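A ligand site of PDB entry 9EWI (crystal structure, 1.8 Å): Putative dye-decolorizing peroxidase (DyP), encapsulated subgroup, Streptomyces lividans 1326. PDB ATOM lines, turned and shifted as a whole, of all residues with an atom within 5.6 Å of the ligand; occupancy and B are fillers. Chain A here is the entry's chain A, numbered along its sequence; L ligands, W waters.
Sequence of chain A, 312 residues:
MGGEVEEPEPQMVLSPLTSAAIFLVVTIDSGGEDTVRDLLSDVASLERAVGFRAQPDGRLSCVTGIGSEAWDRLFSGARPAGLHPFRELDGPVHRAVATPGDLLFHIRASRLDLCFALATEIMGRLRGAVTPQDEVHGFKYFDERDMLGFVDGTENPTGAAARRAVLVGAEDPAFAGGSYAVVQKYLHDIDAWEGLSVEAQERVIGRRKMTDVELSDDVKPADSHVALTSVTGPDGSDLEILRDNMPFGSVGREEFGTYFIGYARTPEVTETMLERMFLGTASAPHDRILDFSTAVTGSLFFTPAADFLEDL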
ATOM      1  N   ASP A 146     -23.764  -0.014 -25.518  1.00  0.00           N
ATOM      2  CA  ASP A 146     -22.668  -0.439 -26.365  1.00  0.00           C
ATOM      3  C   ASP A 146     -23.028  -0.035 -27.769  1.00  0.00           C
ATOM      4  O   ASP A 146     -24.011   0.611 -28.032  1.00  0.00           O
ATOM      5  CB  ASP A 146     -22.359  -1.924 -26.191  1.00  0.00           C
ATOM      6  CG  ASP A 146     -23.498  -2.869 -26.479  1.00  0.00           C
ATOM      7  OD1 ASP A 146     -24.364  -2.498 -27.309  1.00  0.00           O
ATOM      8  OD2 ASP A 146     -23.531  -3.931 -25.783  1.00  0.00           O
ATOM      9  N   LEU A 148     -24.019  -1.741 -30.229  1.00  0.00           N
ATOM     10  CA  LEU A 148     -25.241  -2.306 -30.760  1.00  0.00           C
ATOM     11  C   LEU A 148     -26.475  -1.604 -30.216  1.00  0.00           C
ATOM     12  O   LEU A 148     -27.566  -1.924 -30.598  1.00  0.00           O
ATOM     13  CB  LEU A 148     -25.290  -3.778 -30.376  1.00  0.00           C
ATOM     14  CG  LEU A 148     -24.125  -4.650 -30.855  1.00  0.00           C
ATOM     15  CD1 LEU A 148     -24.269  -6.065 -30.335  1.00  0.00           C
ATOM     16  CD2 LEU A 148     -24.026  -4.627 -32.388  1.00  0.00           C
ATOM     17  N   PHE A 150     -27.557  -1.482 -26.995  1.00  0.00           N
ATOM     18  CA  PHE A 150     -28.097  -2.103 -25.802  1.00  0.00           C
ATOM     19  C   PHE A 150     -27.288  -1.704 -24.570  1.00  0.00           C
ATOM     20  O   PHE A 150     -26.071  -1.501 -24.659  1.00  0.00           O
ATOM     21  CB  PHE A 150     -28.117  -3.609 -25.929  1.00  0.00           C
ATOM     22  CG  PHE A 150     -29.282  -4.100 -26.778  1.00  0.00           C
ATOM     23  CD1 PHE A 150     -29.286  -3.942 -28.138  1.00  0.00           C
ATOM     24  CD2 PHE A 150     -30.331  -4.775 -26.210  1.00  0.00           C
ATOM     25  CE1 PHE A 150     -30.350  -4.400 -28.904  1.00  0.00           C
ATOM     26  CE2 PHE A 150     -31.387  -5.206 -26.964  1.00  0.00           C
ATOM     27  CZ  PHE A 150     -31.409  -5.006 -28.305  1.00  0.00           C
ATOM     28  N   VAL A 151     -27.985  -1.594 -23.413  1.00  0.00           N
ATOM     29  CA  VAL A 151     -27.327  -1.350 -22.144  1.00  0.00           C
ATOM     30  C   VAL A 151     -26.434  -2.562 -21.838  1.00  0.00           C
ATOM     31  O   VAL A 151     -26.877  -3.693 -21.972  1.00  0.00           O
ATOM     32  CB  VAL A 151     -28.323  -1.108 -20.996  1.00  0.00           C
ATOM     33  CG1 VAL A 151     -27.614  -0.893 -19.674  1.00  0.00           C
ATOM     34  CG2 VAL A 151     -29.281   0.043 -21.276  1.00  0.00           C
ATOM     35  N   ASP A 152     -25.204  -2.294 -21.389  1.00  0.00           N
ATOM     36  CA  ASP A 152     -24.134  -3.264 -21.277  1.00  0.00           C
ATOM     37  C   ASP A 152     -23.586  -3.155 -19.841  1.00  0.00           C
ATOM     38  O   ASP A 152     -23.032  -2.127 -19.489  1.00  0.00           O
ATOM     39  CB  ASP A 152     -23.110  -3.012 -22.394  1.00  0.00           C
ATOM     40  CG  ASP A 152     -22.078  -4.131 -22.649  1.00  0.00           C
ATOM     41  OD1 ASP A 152     -21.576  -4.640 -21.600  1.00  0.00           O
ATOM     42  OD2 ASP A 152     -21.756  -4.458 -23.878  1.00  0.00           O
ATOM     43  N   GLY A 153     -23.769  -4.198 -19.038  1.00  0.00           N
ATOM     44  CA  GLY A 153     -23.298  -4.168 -17.651  1.00  0.00           C
ATOM     45  C   GLY A 153     -24.335  -4.600 -16.606  1.00  0.00           C
ATOM     46  O   GLY A 153     -23.987  -4.891 -15.480  1.00  0.00           O
ATOM     47  N   THR A 154     -25.617  -4.654 -16.988  1.00  0.00           N
ATOM     48  CA  THR A 154     -26.741  -4.681 -16.088  1.00  0.00           C
ATOM     49  C   THR A 154     -26.646  -5.847 -15.107  1.00  0.00           C
ATOM     50  O   THR A 154     -26.851  -5.654 -13.916  1.00  0.00           O
ATOM     51  CB  THR A 154     -28.003  -4.828 -16.921  1.00  0.00           C
ATOM     52  OG1 THR A 154     -27.973  -3.781 -17.900  1.00  0.00           O
ATOM     53  CG2 THR A 154     -29.250  -4.677 -16.049  1.00  0.00           C
ATOM     54  N   GLU A 155     -26.359  -7.054 -15.610  1.00  0.00           N
ATOM     55  CA  GLU A 155     -26.330  -8.223 -14.752  1.00  0.00           C
ATOM     56  C   GLU A 155     -24.968  -8.541 -14.168  1.00  0.00           C
ATOM     57  O   GLU A 155     -24.773  -9.593 -13.596  1.00  0.00           O
ATOM     58  CB  GLU A 155     -26.927  -9.404 -15.508  1.00  0.00           C
ATOM     59  CG  GLU A 155     -28.465  -9.326 -15.610  1.00  0.00           C
ATOM     60  CD  GLU A 155     -29.183  -9.328 -14.274  1.00  0.00           C
ATOM     61  OE1 GLU A 155     -28.941 -10.298 -13.565  1.00  0.00           O
ATOM     62  OE2 GLU A 155     -29.910  -8.389 -13.934  1.00  0.00           O
ATOM     63  N   ASN A 156     -24.017  -7.626 -14.205  1.00  0.00           N
ATOM     64  CA  ASN A 156     -22.761  -7.872 -13.533  1.00  0.00           C
ATOM     65  C   ASN A 156     -23.019  -8.083 -12.056  1.00  0.00           C
ATOM     66  O   ASN A 156     -23.842  -7.369 -11.491  1.00  0.00           O
ATOM     67  CB  ASN A 156     -21.784  -6.711 -13.621  1.00  0.00           C
ATOM     68  CG  ASN A 156     -20.848  -6.855 -14.791  1.00  0.00           C
ATOM     69  OD1 ASN A 156     -20.442  -7.980 -15.155  1.00  0.00           O
ATOM     70  ND2 ASN A 156     -20.505  -5.749 -15.419  1.00  0.00           N
ATOM     71  N   GLN A 184     -11.102  -9.911 -25.518  1.00  0.00           N
ATOM     72  CA  GLN A 184     -11.316 -10.062 -26.937  1.00  0.00           C
ATOM     73  C   GLN A 184     -11.765  -8.731 -27.547  1.00  0.00           C
ATOM     74  O   GLN A 184     -12.688  -8.092 -27.051  1.00  0.00           O
ATOM     75  CB  GLN A 184     -12.446 -11.040 -27.162  1.00  0.00           C
ATOM     76  CG  GLN A 184     -12.158 -12.484 -26.794  1.00  0.00           C
ATOM     77  CD  GLN A 184     -13.370 -13.309 -27.093  1.00  0.00           C
ATOM     78  OE1 GLN A 184     -14.435 -13.097 -26.499  1.00  0.00           O
ATOM     79  NE2 GLN A 184     -13.234 -14.166 -28.096  1.00  0.00           N
ATOM     80  N   TYR A 186     -13.742  -7.069 -30.393  1.00  0.00           N
ATOM     81  CA  TYR A 186     -14.748  -7.408 -31.378  1.00  0.00           C
ATOM     82  C   TYR A 186     -15.031  -6.199 -32.275  1.00  0.00           C
ATOM     83  O   TYR A 186     -15.187  -5.082 -31.790  1.00  0.00           O
ATOM     84  CB  TYR A 186     -16.080  -7.779 -30.706  1.00  0.00           C
ATOM     85  CG  TYR A 186     -16.119  -9.177 -30.122  1.00  0.00           C
ATOM     86  CD1 TYR A 186     -16.507 -10.274 -30.879  1.00  0.00           C
ATOM     87  CD2 TYR A 186     -15.787  -9.382 -28.779  1.00  0.00           C
ATOM     88  CE1 TYR A 186     -16.585 -11.533 -30.319  1.00  0.00           C
ATOM     89  CE2 TYR A 186     -15.786 -10.648 -28.232  1.00  0.00           C
ATOM     90  CZ  TYR A 186     -16.224 -11.737 -28.997  1.00  0.00           C
ATOM     91  OH  TYR A 186     -16.314 -12.978 -28.396  1.00  0.00           O
ATOM     92  N   HIS A 188     -18.020  -4.942 -35.056  1.00  0.00           N
ATOM     93  CA  HIS A 188     -19.400  -5.200 -35.380  1.00  0.00           C
ATOM     94  C   HIS A 188     -19.666  -4.817 -36.826  1.00  0.00           C
ATOM     95  O   HIS A 188     -19.109  -3.862 -37.324  1.00  0.00           O
ATOM     96  CB  HIS A 188     -20.337  -4.433 -34.461  1.00  0.00           C
ATOM     97  CG  HIS A 188     -20.178  -4.813 -33.047  1.00  0.00           C
ATOM     98  ND1 HIS A 188     -20.545  -6.059 -32.594  1.00  0.00           N
ATOM     99  CD2 HIS A 188     -19.707  -4.123 -31.992  1.00  0.00           C
ATOM    100  CE1 HIS A 188     -20.307  -6.097 -31.275  1.00  0.00           C
ATOM    101  NE2 HIS A 188     -19.814  -4.922 -30.877  1.00  0.00           N
ATOM    102  N   ILE A 205     -30.190 -10.484 -28.391  1.00  0.00           N
ATOM    103  CA  ILE A 205     -29.561 -10.199 -27.115  1.00  0.00           C
ATOM    104  C   ILE A 205     -30.249 -10.961 -25.988  1.00  0.00           C
ATOM    105  O   ILE A 205     -29.568 -11.530 -25.153  1.00  0.00           O
ATOM    106  CB  ILE A 205     -29.587  -8.686 -26.852  1.00  0.00           C
ATOM    107  CG1 ILE A 205     -28.847  -7.911 -27.917  1.00  0.00           C
ATOM    108  CG2 ILE A 205     -29.050  -8.326 -25.454  1.00  0.00           C
ATOM    109  CD1 ILE A 205     -27.372  -8.231 -28.015  1.00  0.00           C
ATOM    110  N   ARG A 207     -32.832  -9.201 -24.141  1.00  0.00           N
ATOM    111  CA  ARG A 207     -33.410  -8.175 -23.306  1.00  0.00           C
ATOM    112  C   ARG A 207     -34.079  -7.140 -24.189  1.00  0.00           C
ATOM    113  O   ARG A 207     -33.776  -7.043 -25.354  1.00  0.00           O
ATOM    114  CB  ARG A 207     -32.306  -7.454 -22.516  1.00  0.00           C
ATOM    115  CG  ARG A 207     -31.418  -8.409 -21.726  1.00  0.00           C
ATOM    116  CD  ARG A 207     -30.407  -7.713 -20.872  1.00  0.00           C
ATOM    117  NE  ARG A 207     -30.976  -6.980 -19.733  1.00  0.00           N
ATOM    118  CZ  ARG A 207     -31.233  -7.479 -18.523  1.00  0.00           C
ATOM    119  NH1 ARG A 207     -30.864  -8.682 -18.185  1.00  0.00           N
ATOM    120  NH2 ARG A 207     -31.849  -6.753 -17.608  1.00  0.00           N
ATOM    121  N   ASP A 212     -34.259  -2.216 -21.162  1.00  0.00           N
ATOM    122  CA  ASP A 212     -33.308  -3.131 -20.550  1.00  0.00           C
ATOM    123  C   ASP A 212     -33.955  -4.146 -19.596  1.00  0.00           C
ATOM    124  O   ASP A 212     -33.323  -4.653 -18.689  1.00  0.00           O
ATOM    125  CB  ASP A 212     -32.186  -2.398 -19.821  1.00  0.00           C
ATOM    126  CG  ASP A 212     -30.930  -3.230 -19.565  1.00  0.00           C
ATOM    127  OD1 ASP A 212     -30.694  -4.254 -20.303  1.00  0.00           O
ATOM    128  OD2 ASP A 212     -30.197  -2.830 -18.653  1.00  0.00           O
ATOM    129  N   GLU A 214     -35.208  -7.899 -19.008  1.00  0.00           N
ATOM    130  CA  GLU A 214     -34.966  -9.205 -19.590  1.00  0.00           C
ATOM    131  C   GLU A 214     -36.232  -9.768 -20.242  1.00  0.00           C
ATOM    132  O   GLU A 214     -37.324  -9.571 -19.766  1.00  0.00           O
ATOM    133  CB  GLU A 214     -34.426 -10.048 -18.443  1.00  0.00           C
ATOM    134  CG  GLU A 214     -34.058 -11.461 -18.853  1.00  0.00           C
ATOM    135  CD  GLU A 214     -33.217 -12.149 -17.796  1.00  0.00           C
ATOM    136  OE1 GLU A 214     -32.818 -11.562 -16.768  1.00  0.00           O
ATOM    137  OE2 GLU A 214     -32.845 -13.255 -18.130  1.00  0.00           O
ATOM    138  N   HIS A 225     -27.936 -14.200 -26.608  1.00  0.00           N
ATOM    139  CA  HIS A 225     -26.681 -13.987 -25.887  1.00  0.00           C
ATOM    140  C   HIS A 225     -26.854 -14.246 -24.388  1.00  0.00           C
ATOM    141  O   HIS A 225     -25.999 -14.900 -23.756  1.00  0.00           O
ATOM    142  CB  HIS A 225     -26.157 -12.571 -26.171  1.00  0.00           C
ATOM    143  CG  HIS A 225     -24.891 -12.256 -25.502  1.00  0.00           C
ATOM    144  ND1 HIS A 225     -23.754 -12.977 -25.747  1.00  0.00           N
ATOM    145  CD2 HIS A 225     -24.546 -11.271 -24.676  1.00  0.00           C
ATOM    146  CE1 HIS A 225     -22.758 -12.435 -25.042  1.00  0.00           C
ATOM    147  NE2 HIS A 225     -23.217 -11.399 -24.378  1.00  0.00           N
ATOM    148  N   VAL A 226     -27.963 -13.742 -23.847  1.00  0.00           N
ATOM    149  CA  VAL A 226     -28.231 -13.884 -22.438  1.00  0.00           C
ATOM    150  C   VAL A 226     -28.511 -15.354 -22.078  1.00  0.00           C
ATOM    151  O   VAL A 226     -28.141 -15.820 -21.011  1.00  0.00           O
ATOM    152  CB  VAL A 226     -29.358 -12.927 -21.995  1.00  0.00           C
ATOM    153  CG1 VAL A 226     -30.027 -13.401 -20.713  1.00  0.00           C
ATOM    154  CG2 VAL A 226     -28.789 -11.506 -21.879  1.00  0.00           C
ATOM    155  N   THR A 229     -25.000 -17.254 -22.137  1.00  0.00           N
ATOM    156  CA  THR A 229     -23.981 -16.855 -21.167  1.00  0.00           C
ATOM    157  C   THR A 229     -24.512 -16.983 -19.734  1.00  0.00           C
ATOM    158  O   THR A 229     -23.828 -16.579 -18.798  1.00  0.00           O
ATOM    159  CB  THR A 229     -23.470 -15.445 -21.454  1.00  0.00           C
ATOM    160  OG1 THR A 229     -24.555 -14.516 -21.421  1.00  0.00           O
ATOM    161  CG2 THR A 229     -22.740 -15.358 -22.784  1.00  0.00           C
ATOM    162  N   SER A 230     -25.711 -17.557 -19.551  1.00  0.00           N
ATOM    163  CA  SER A 230     -26.203 -17.960 -18.244  1.00  0.00           C
ATOM    164  C   SER A 230     -25.813 -19.407 -17.986  1.00  0.00           C
ATOM    165  O   SER A 230     -26.196 -20.283 -18.751  1.00  0.00           O
ATOM    166  CB  SER A 230     -27.684 -17.819 -18.152  1.00  0.00           C
ATOM    167  OG  SER A 230     -28.003 -16.456 -18.327  1.00  0.00           O
ATOM    168  N   ILE A 241     -19.243 -13.822 -13.987  1.00  0.00           N
ATOM    169  CA  ILE A 241     -18.029 -13.071 -14.264  1.00  0.00           C
ATOM    170  C   ILE A 241     -18.303 -11.578 -14.135  1.00  0.00           C
ATOM    171  O   ILE A 241     -19.435 -11.141 -14.121  1.00  0.00           O
ATOM    172  CB  ILE A 241     -17.446 -13.406 -15.648  1.00  0.00           C
ATOM    173  CG1 ILE A 241     -18.257 -12.849 -16.788  1.00  0.00           C
ATOM    174  CG2 ILE A 241     -17.244 -14.919 -15.809  1.00  0.00           C
ATOM    175  CD1 ILE A 241     -17.605 -13.052 -18.133  1.00  0.00           C
ATOM    176  N   ARG A 243     -17.643  -8.094 -16.080  1.00  0.00           N
ATOM    177  CA  ARG A 243     -17.309  -7.549 -17.367  1.00  0.00           C
ATOM    178  C   ARG A 243     -17.206  -6.033 -17.267  1.00  0.00           C
ATOM    179  O   ARG A 243     -17.869  -5.406 -16.453  1.00  0.00           O
ATOM    180  CB  ARG A 243     -18.383  -7.891 -18.398  1.00  0.00           C
ATOM    181  CG  ARG A 243     -18.572  -9.375 -18.606  1.00  0.00           C
ATOM    182  CD  ARG A 243     -19.807  -9.679 -19.391  1.00  0.00           C
ATOM    183  NE  ARG A 243     -20.976  -9.503 -18.528  1.00  0.00           N
ATOM    184  CZ  ARG A 243     -21.988  -8.634 -18.731  1.00  0.00           C
ATOM    185  NH1 ARG A 243     -22.070  -7.953 -19.861  1.00  0.00           N
ATOM    186  NH2 ARG A 243     -22.952  -8.489 -17.815  1.00  0.00           N
ATOM    187  N   ASN A 245     -16.992  -4.087 -20.506  1.00  0.00           N
ATOM    188  CA  ASN A 245     -16.890  -3.891 -21.947  1.00  0.00           C
ATOM    189  C   ASN A 245     -16.913  -2.389 -22.296  1.00  0.00           C
ATOM    190  O   ASN A 245     -17.673  -1.607 -21.699  1.00  0.00           O
ATOM    191  CB  ASN A 245     -18.086  -4.516 -22.660  1.00  0.00           C
ATOM    192  CG  ASN A 245     -18.180  -6.008 -22.450  1.00  0.00           C
ATOM    193  OD1 ASN A 245     -17.245  -6.655 -21.958  1.00  0.00           O
ATOM    194  ND2 ASN A 245     -19.322  -6.560 -22.842  1.00  0.00           N
ATOM    195  N   THR A 258     -16.582  -3.382 -29.769  1.00  0.00           N
ATOM    196  CA  THR A 258     -16.733  -3.607 -28.332  1.00  0.00           C
ATOM    197  C   THR A 258     -15.455  -4.271 -27.886  1.00  0.00           C
ATOM    198  O   THR A 258     -15.072  -5.283 -28.452  1.00  0.00           O
ATOM    199  CB  THR A 258     -17.975  -4.475 -28.033  1.00  0.00           C
ATOM    200  OG1 THR A 258     -19.206  -3.820 -28.394  1.00  0.00           O
ATOM    201  CG2 THR A 258     -17.996  -4.964 -26.584  1.00  0.00           C
ATOM    202  N   PHE A 260     -14.105  -6.448 -25.188  1.00  0.00           N
ATOM    203  CA  PHE A 260     -14.616  -7.300 -24.135  1.00  0.00           C
ATOM    204  C   PHE A 260     -13.492  -7.591 -23.132  1.00  0.00           C
ATOM    205  O   PHE A 260     -12.395  -7.953 -23.552  1.00  0.00           O
ATOM    206  CB  PHE A 260     -15.105  -8.626 -24.702  1.00  0.00           C
ATOM    207  CG  PHE A 260     -15.374  -9.639 -23.611  1.00  0.00           C
ATOM    208  CD1 PHE A 260     -16.557  -9.609 -22.916  1.00  0.00           C
ATOM    209  CD2 PHE A 260     -14.441 -10.588 -23.280  1.00  0.00           C
ATOM    210  CE1 PHE A 260     -16.819 -10.550 -21.934  1.00  0.00           C
ATOM    211  CE2 PHE A 260     -14.702 -11.492 -22.281  1.00  0.00           C
ATOM    212  CZ  PHE A 260     -15.878 -11.465 -21.609  1.00  0.00           C
ATOM    213  N   THR A 270     -15.219 -18.419 -17.590  1.00  0.00           N
ATOM    214  CA  THR A 270     -15.226 -17.617 -18.806  1.00  0.00           C
ATOM    215  C   THR A 270     -15.152 -18.508 -20.013  1.00  0.00           C
ATOM    216  O   THR A 270     -15.854 -18.277 -20.995  1.00  0.00           O
ATOM    217  CB  THR A 270     -14.058 -16.652 -18.773  1.00  0.00           C
ATOM    218  OG1 THR A 270     -14.110 -15.924 -17.552  1.00  0.00           O
ATOM    219  CG2 THR A 270     -14.198 -15.589 -19.824  1.00  0.00           C
ATOM    220  N   MET A 273     -18.485 -20.191 -20.946  1.00  0.00           N
ATOM    221  CA  MET A 273     -19.336 -19.250 -21.654  1.00  0.00           C
ATOM    222  C   MET A 273     -18.873 -19.137 -23.107  1.00  0.00           C
ATOM    223  O   MET A 273     -19.681 -19.140 -24.033  1.00  0.00           O
ATOM    224  CB  MET A 273     -19.305 -17.899 -20.959  1.00  0.00           C
ATOM    225  CG  MET A 273     -19.976 -17.885 -19.615  1.00  0.00           C
ATOM    226  SD  MET A 273     -19.684 -16.305 -18.799  1.00  0.00           S
ATOM    227  CE  MET A 273     -20.645 -16.520 -17.288  1.00  0.00           C
ATOM    228  N   LEU A 274     -17.579 -19.028 -23.317  1.00  0.00           N
ATOM    229  CA  LEU A 274     -17.079 -18.888 -24.680  1.00  0.00           C
ATOM    230  C   LEU A 274     -17.395 -20.108 -25.538  1.00  0.00           C
ATOM    231  O   LEU A 274     -17.676 -19.966 -26.732  1.00  0.00           O
ATOM    232  CB  LEU A 274     -15.577 -18.645 -24.626  1.00  0.00           C
ATOM    233  CG  LEU A 274     -15.112 -17.227 -24.314  1.00  0.00           C
ATOM    234  CD1 LEU A 274     -13.606 -17.195 -24.105  1.00  0.00           C
ATOM    235  CD2 LEU A 274     -15.464 -16.330 -25.478  1.00  0.00           C
ATOM    236  N   MET A 277     -20.903 -19.969 -26.595  1.00  0.00           N
ATOM    237  CA  MET A 277     -21.149 -18.969 -27.611  1.00  0.00           C
ATOM    238  C   MET A 277     -20.643 -19.454 -28.967  1.00  0.00           C
ATOM    239  O   MET A 277     -21.334 -19.259 -29.954  1.00  0.00           O
ATOM    240  CB  MET A 277     -20.473 -17.635 -27.258  1.00  0.00           C
ATOM    241  CG  MET A 277     -21.078 -16.905 -26.065  1.00  0.00           C
ATOM    242  SD  MET A 277     -20.026 -15.470 -25.639  1.00  0.00           S
ATOM    243  CE  MET A 277     -20.176 -14.471 -27.106  1.00  0.00           C
ATOM    244  N   ILE A 289     -25.274 -13.162 -31.344  1.00  0.00           N
ATOM    245  CA  ILE A 289     -24.521 -11.932 -31.358  1.00  0.00           C
ATOM    246  C   ILE A 289     -23.292 -12.056 -32.273  1.00  0.00           C
ATOM    247  O   ILE A 289     -22.833 -11.060 -32.819  1.00  0.00           O
ATOM    248  CB  ILE A 289     -24.145 -11.534 -29.911  1.00  0.00           C
ATOM    249  CG1 ILE A 289     -23.995 -10.055 -29.762  1.00  0.00           C
ATOM    250  CG2 ILE A 289     -22.854 -12.195 -29.454  1.00  0.00           C
ATOM    251  CD1 ILE A 289     -23.803  -9.552 -28.345  1.00  0.00           C
ATOM    252  N   LEU A 290     -22.752 -13.272 -32.435  1.00  0.00           N
ATOM    253  CA  LEU A 290     -21.579 -13.490 -33.262  1.00  0.00           C
ATOM    254  C   LEU A 290     -21.890 -13.380 -34.759  1.00  0.00           C
ATOM    255  O   LEU A 290     -20.995 -13.235 -35.563  1.00  0.00           O
ATOM    256  CB  LEU A 290     -20.975 -14.855 -32.952  1.00  0.00           C
ATOM    257  CG  LEU A 290     -20.450 -15.027 -31.538  1.00  0.00           C
ATOM    258  CD1 LEU A 290     -19.933 -16.456 -31.402  1.00  0.00           C
ATOM    259  CD2 LEU A 290     -19.345 -14.059 -31.228  1.00  0.00           C
ATOM    260  N   SER A 293     -20.721  -9.821 -34.975  1.00  0.00           N
ATOM    261  CA  SER A 293     -19.568  -9.485 -34.155  1.00  0.00           C
ATOM    262  C   SER A 293     -18.437 -10.462 -34.508  1.00  0.00           C
ATOM    263  O   SER A 293     -18.619 -11.658 -34.382  1.00  0.00           O
ATOM    264  CB  SER A 293     -19.908  -9.536 -32.671  1.00  0.00           C
ATOM    265  OG  SER A 293     -21.126  -8.876 -32.367  1.00  0.00           O
HETATM  266  C1  LIG L   1     -24.717  -9.829 -21.007  1.00  0.00           C
HETATM  267  C2  LIG L   1     -23.210  -7.365 -24.862  1.00  0.00           C
HETATM  268  C3  LIG L   1     -19.479 -10.487 -25.421  1.00  0.00           C
HETATM  269  C4  LIG L   1     -20.823 -12.573 -21.256  1.00  0.00           C
HETATM  270  C5  LIG L   1     -24.636  -8.922 -22.040  1.00  0.00           C
HETATM  271  C6  LIG L   1     -25.665  -7.961 -22.333  1.00  0.00           C
HETATM  272  C7  LIG L   1     -25.221  -7.236 -23.413  1.00  0.00           C
HETATM  273  C8  LIG L   1     -23.984  -7.785 -23.820  1.00  0.00           C
HETATM  274  C9  LIG L   1     -25.949  -6.085 -24.066  1.00  0.00           C
HETATM  275  C10 LIG L   1     -26.962  -7.760 -21.560  1.00  0.00           C
HETATM  276  C11 LIG L   1     -26.806  -6.731 -20.384  1.00  0.00           C
HETATM  277  C12 LIG L   1     -25.807  -7.151 -19.366  1.00  0.00           C
HETATM  278  O1  LIG L   1     -24.631  -6.781 -19.466  1.00  0.00           O
HETATM  279  O2  LIG L   1     -26.223  -7.903 -18.441  1.00  0.00           O
HETATM  280  C13 LIG L   1     -22.073  -7.985 -25.346  1.00  0.00           C
HETATM  281  C14 LIG L   1     -21.382  -7.590 -26.522  1.00  0.00           C
HETATM  282  C15 LIG L   1     -20.294  -8.410 -26.692  1.00  0.00           C
HETATM  283  C16 LIG L   1     -20.378  -9.434 -25.603  1.00  0.00           C
HETATM  284  C17 LIG L   1     -21.662  -6.382 -27.397  1.00  0.00           C
HETATM  285  C18 LIG L   1     -19.430  -8.301 -27.889  1.00  0.00           C
HETATM  286  C19 LIG L   1     -19.426  -9.356 -28.677  1.00  0.00           C
HETATM  287  C20 LIG L   1     -19.507 -11.336 -24.327  1.00  0.00           C
HETATM  288  C21 LIG L   1     -18.632 -12.431 -24.087  1.00  0.00           C
HETATM  289  C22 LIG L   1     -19.020 -13.059 -22.906  1.00  0.00           C
HETATM  290  C23 LIG L   1     -20.158 -12.312 -22.450  1.00  0.00           C
HETATM  291  C24 LIG L   1     -17.486 -12.785 -25.022  1.00  0.00           C
HETATM  292  C25 LIG L   1     -18.497 -14.181 -22.109  1.00  0.00           C
HETATM  293  C26 LIG L   1     -17.411 -14.843 -22.394  1.00  0.00           C
HETATM  294  C27 LIG L   1     -21.970 -11.959 -20.852  1.00  0.00           C
HETATM  295  C28 LIG L   1     -22.597 -12.331 -19.620  1.00  0.00           C
HETATM  296  C29 LIG L   1     -23.720 -11.594 -19.566  1.00  0.00           C
HETATM  297  C30 LIG L   1     -23.706 -10.752 -20.785  1.00  0.00           C
HETATM  298  C31 LIG L   1     -22.148 -13.350 -18.600  1.00  0.00           C
HETATM  299  C32 LIG L   1     -24.769 -11.577 -18.468  1.00  0.00           C
HETATM  300  C33 LIG L   1     -25.824 -12.708 -18.686  1.00  0.00           C
HETATM  301  C34 LIG L   1     -26.889 -12.805 -17.553  1.00  0.00           C
HETATM  302  O3  LIG L   1     -26.780 -13.518 -16.570  1.00  0.00           O
HETATM  303  O4  LIG L   1     -27.946 -12.157 -17.550  1.00  0.00           O
HETATM  304  N1  LIG L   1     -23.628  -8.799 -22.996  1.00  0.00           N
HETATM  305  N2  LIG L   1     -21.465  -9.089 -24.860  1.00  0.00           N
HETATM  306  N3  LIG L   1     -20.400 -11.279 -23.318  1.00  0.00           N
HETATM  307  N4  LIG L   1     -22.636 -11.000 -21.527  1.00  0.00           N
HETATM  308 FE1  LIG L   1     -22.106 -10.108 -23.169  1.00  0.00          FE
HETATM  309  O   HOH W   1     -24.150 -14.785 -16.589  1.00  0.00           O
HETATM  310  O   HOH W   2     -28.200  -9.854 -19.063  1.00  0.00           O
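A ring nitrogen (NE2) of His 225 is bound to an iron atom (FE1) of the ligand (2.1 Å). N of Gly 153 sits at hydrogen-bond distance from O1 of the ligand, at 2.8 Å. An oxygen (O1) of the ligand is in salt-bridge range of the guanidinium group (NH1) of Arg 243 (2.8 Å). O2 of the ligand is in hydrogen-bond range of N of Glu 155 (3.0 Å). The backbone NH (N) of Thr 154 is in hydrogen-bond range of an oxygen (O1) of the ligand (3.4 Å).
Residues that only touch the ligand: Asp 146 (3.5 Å), Leu 148 (3.9 Å), Phe 150 (3.8 Å), Val 151 (3.3 Å), Asp 152 (3.4 Å), Gln 184 (3.4 Å), Tyr 186 (3.6 Å), Arg 207 (3.5 Å), Val 226 (3.99 Å), Thr 229 (3.4 Å), Ser 230 (3.6 Å), Asn 245 (3.9 Å), Thr 258 (3.7 Å), Phe 260 (3.4 Å), Met 273 (3.7 Å), Leu 274 (3.8 Å), Met 277 (3.7 Å) and Ile 289 (3.6 Å). Within 4 Å of the ligand: Asp 146, Leu 148, Phe 150, Val 151, Asp 152, Gly 153, Thr 154, Glu 155, Gln 184, Tyr 186, Arg 207, His 225, Val 226, Thr 229, Ser 230, Arg 243, Asn 245, Thr 258, Phe 260, Met 273, Leu 274, Met 277 and Ile 289. The nearest printed residue that does not touch the ligand is Thr 270 (4.02 Å).
OD1 of Asp 152 is in salt-bridge range of NH1 of Arg 243 (3.8 Å). The side-chain amide oxygen (OE1) of Gln 184 lies within hydrogen-bond range of the side-chain hydroxyl (OH) of Tyr 186 (2.7 Å). OD1 of Asp 146 lies within hydrogen-bond range of N of Phe 150, 3.4 Å away. The side-chain carboxylate of Asp 212 is in salt-bridge range of the guanidinium group of Arg 207. OE1 of Glu 214 is in salt-bridge range of NH1 of Arg 207. The backbone carbonyl oxygen (O) of Ile 289 lies within hydrogen-bond range of the side-chain hydroxyl (OG) of Ser 293. The side-chain hydroxyl (OG1) of Thr 258 is in hydrogen-bond range of a ring nitrogen (NE2) of His 188. The backbone carbonyl oxygen of Ile 205 lies within hydrogen-bond range of the backbone NH of Val 226.
Water W2 lies within hydrogen-bond range of O4 of the ligand and NH1 of Arg 207. Water W1 lies within hydrogen-bond range of O of Thr 229 and O3 of the ligand.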
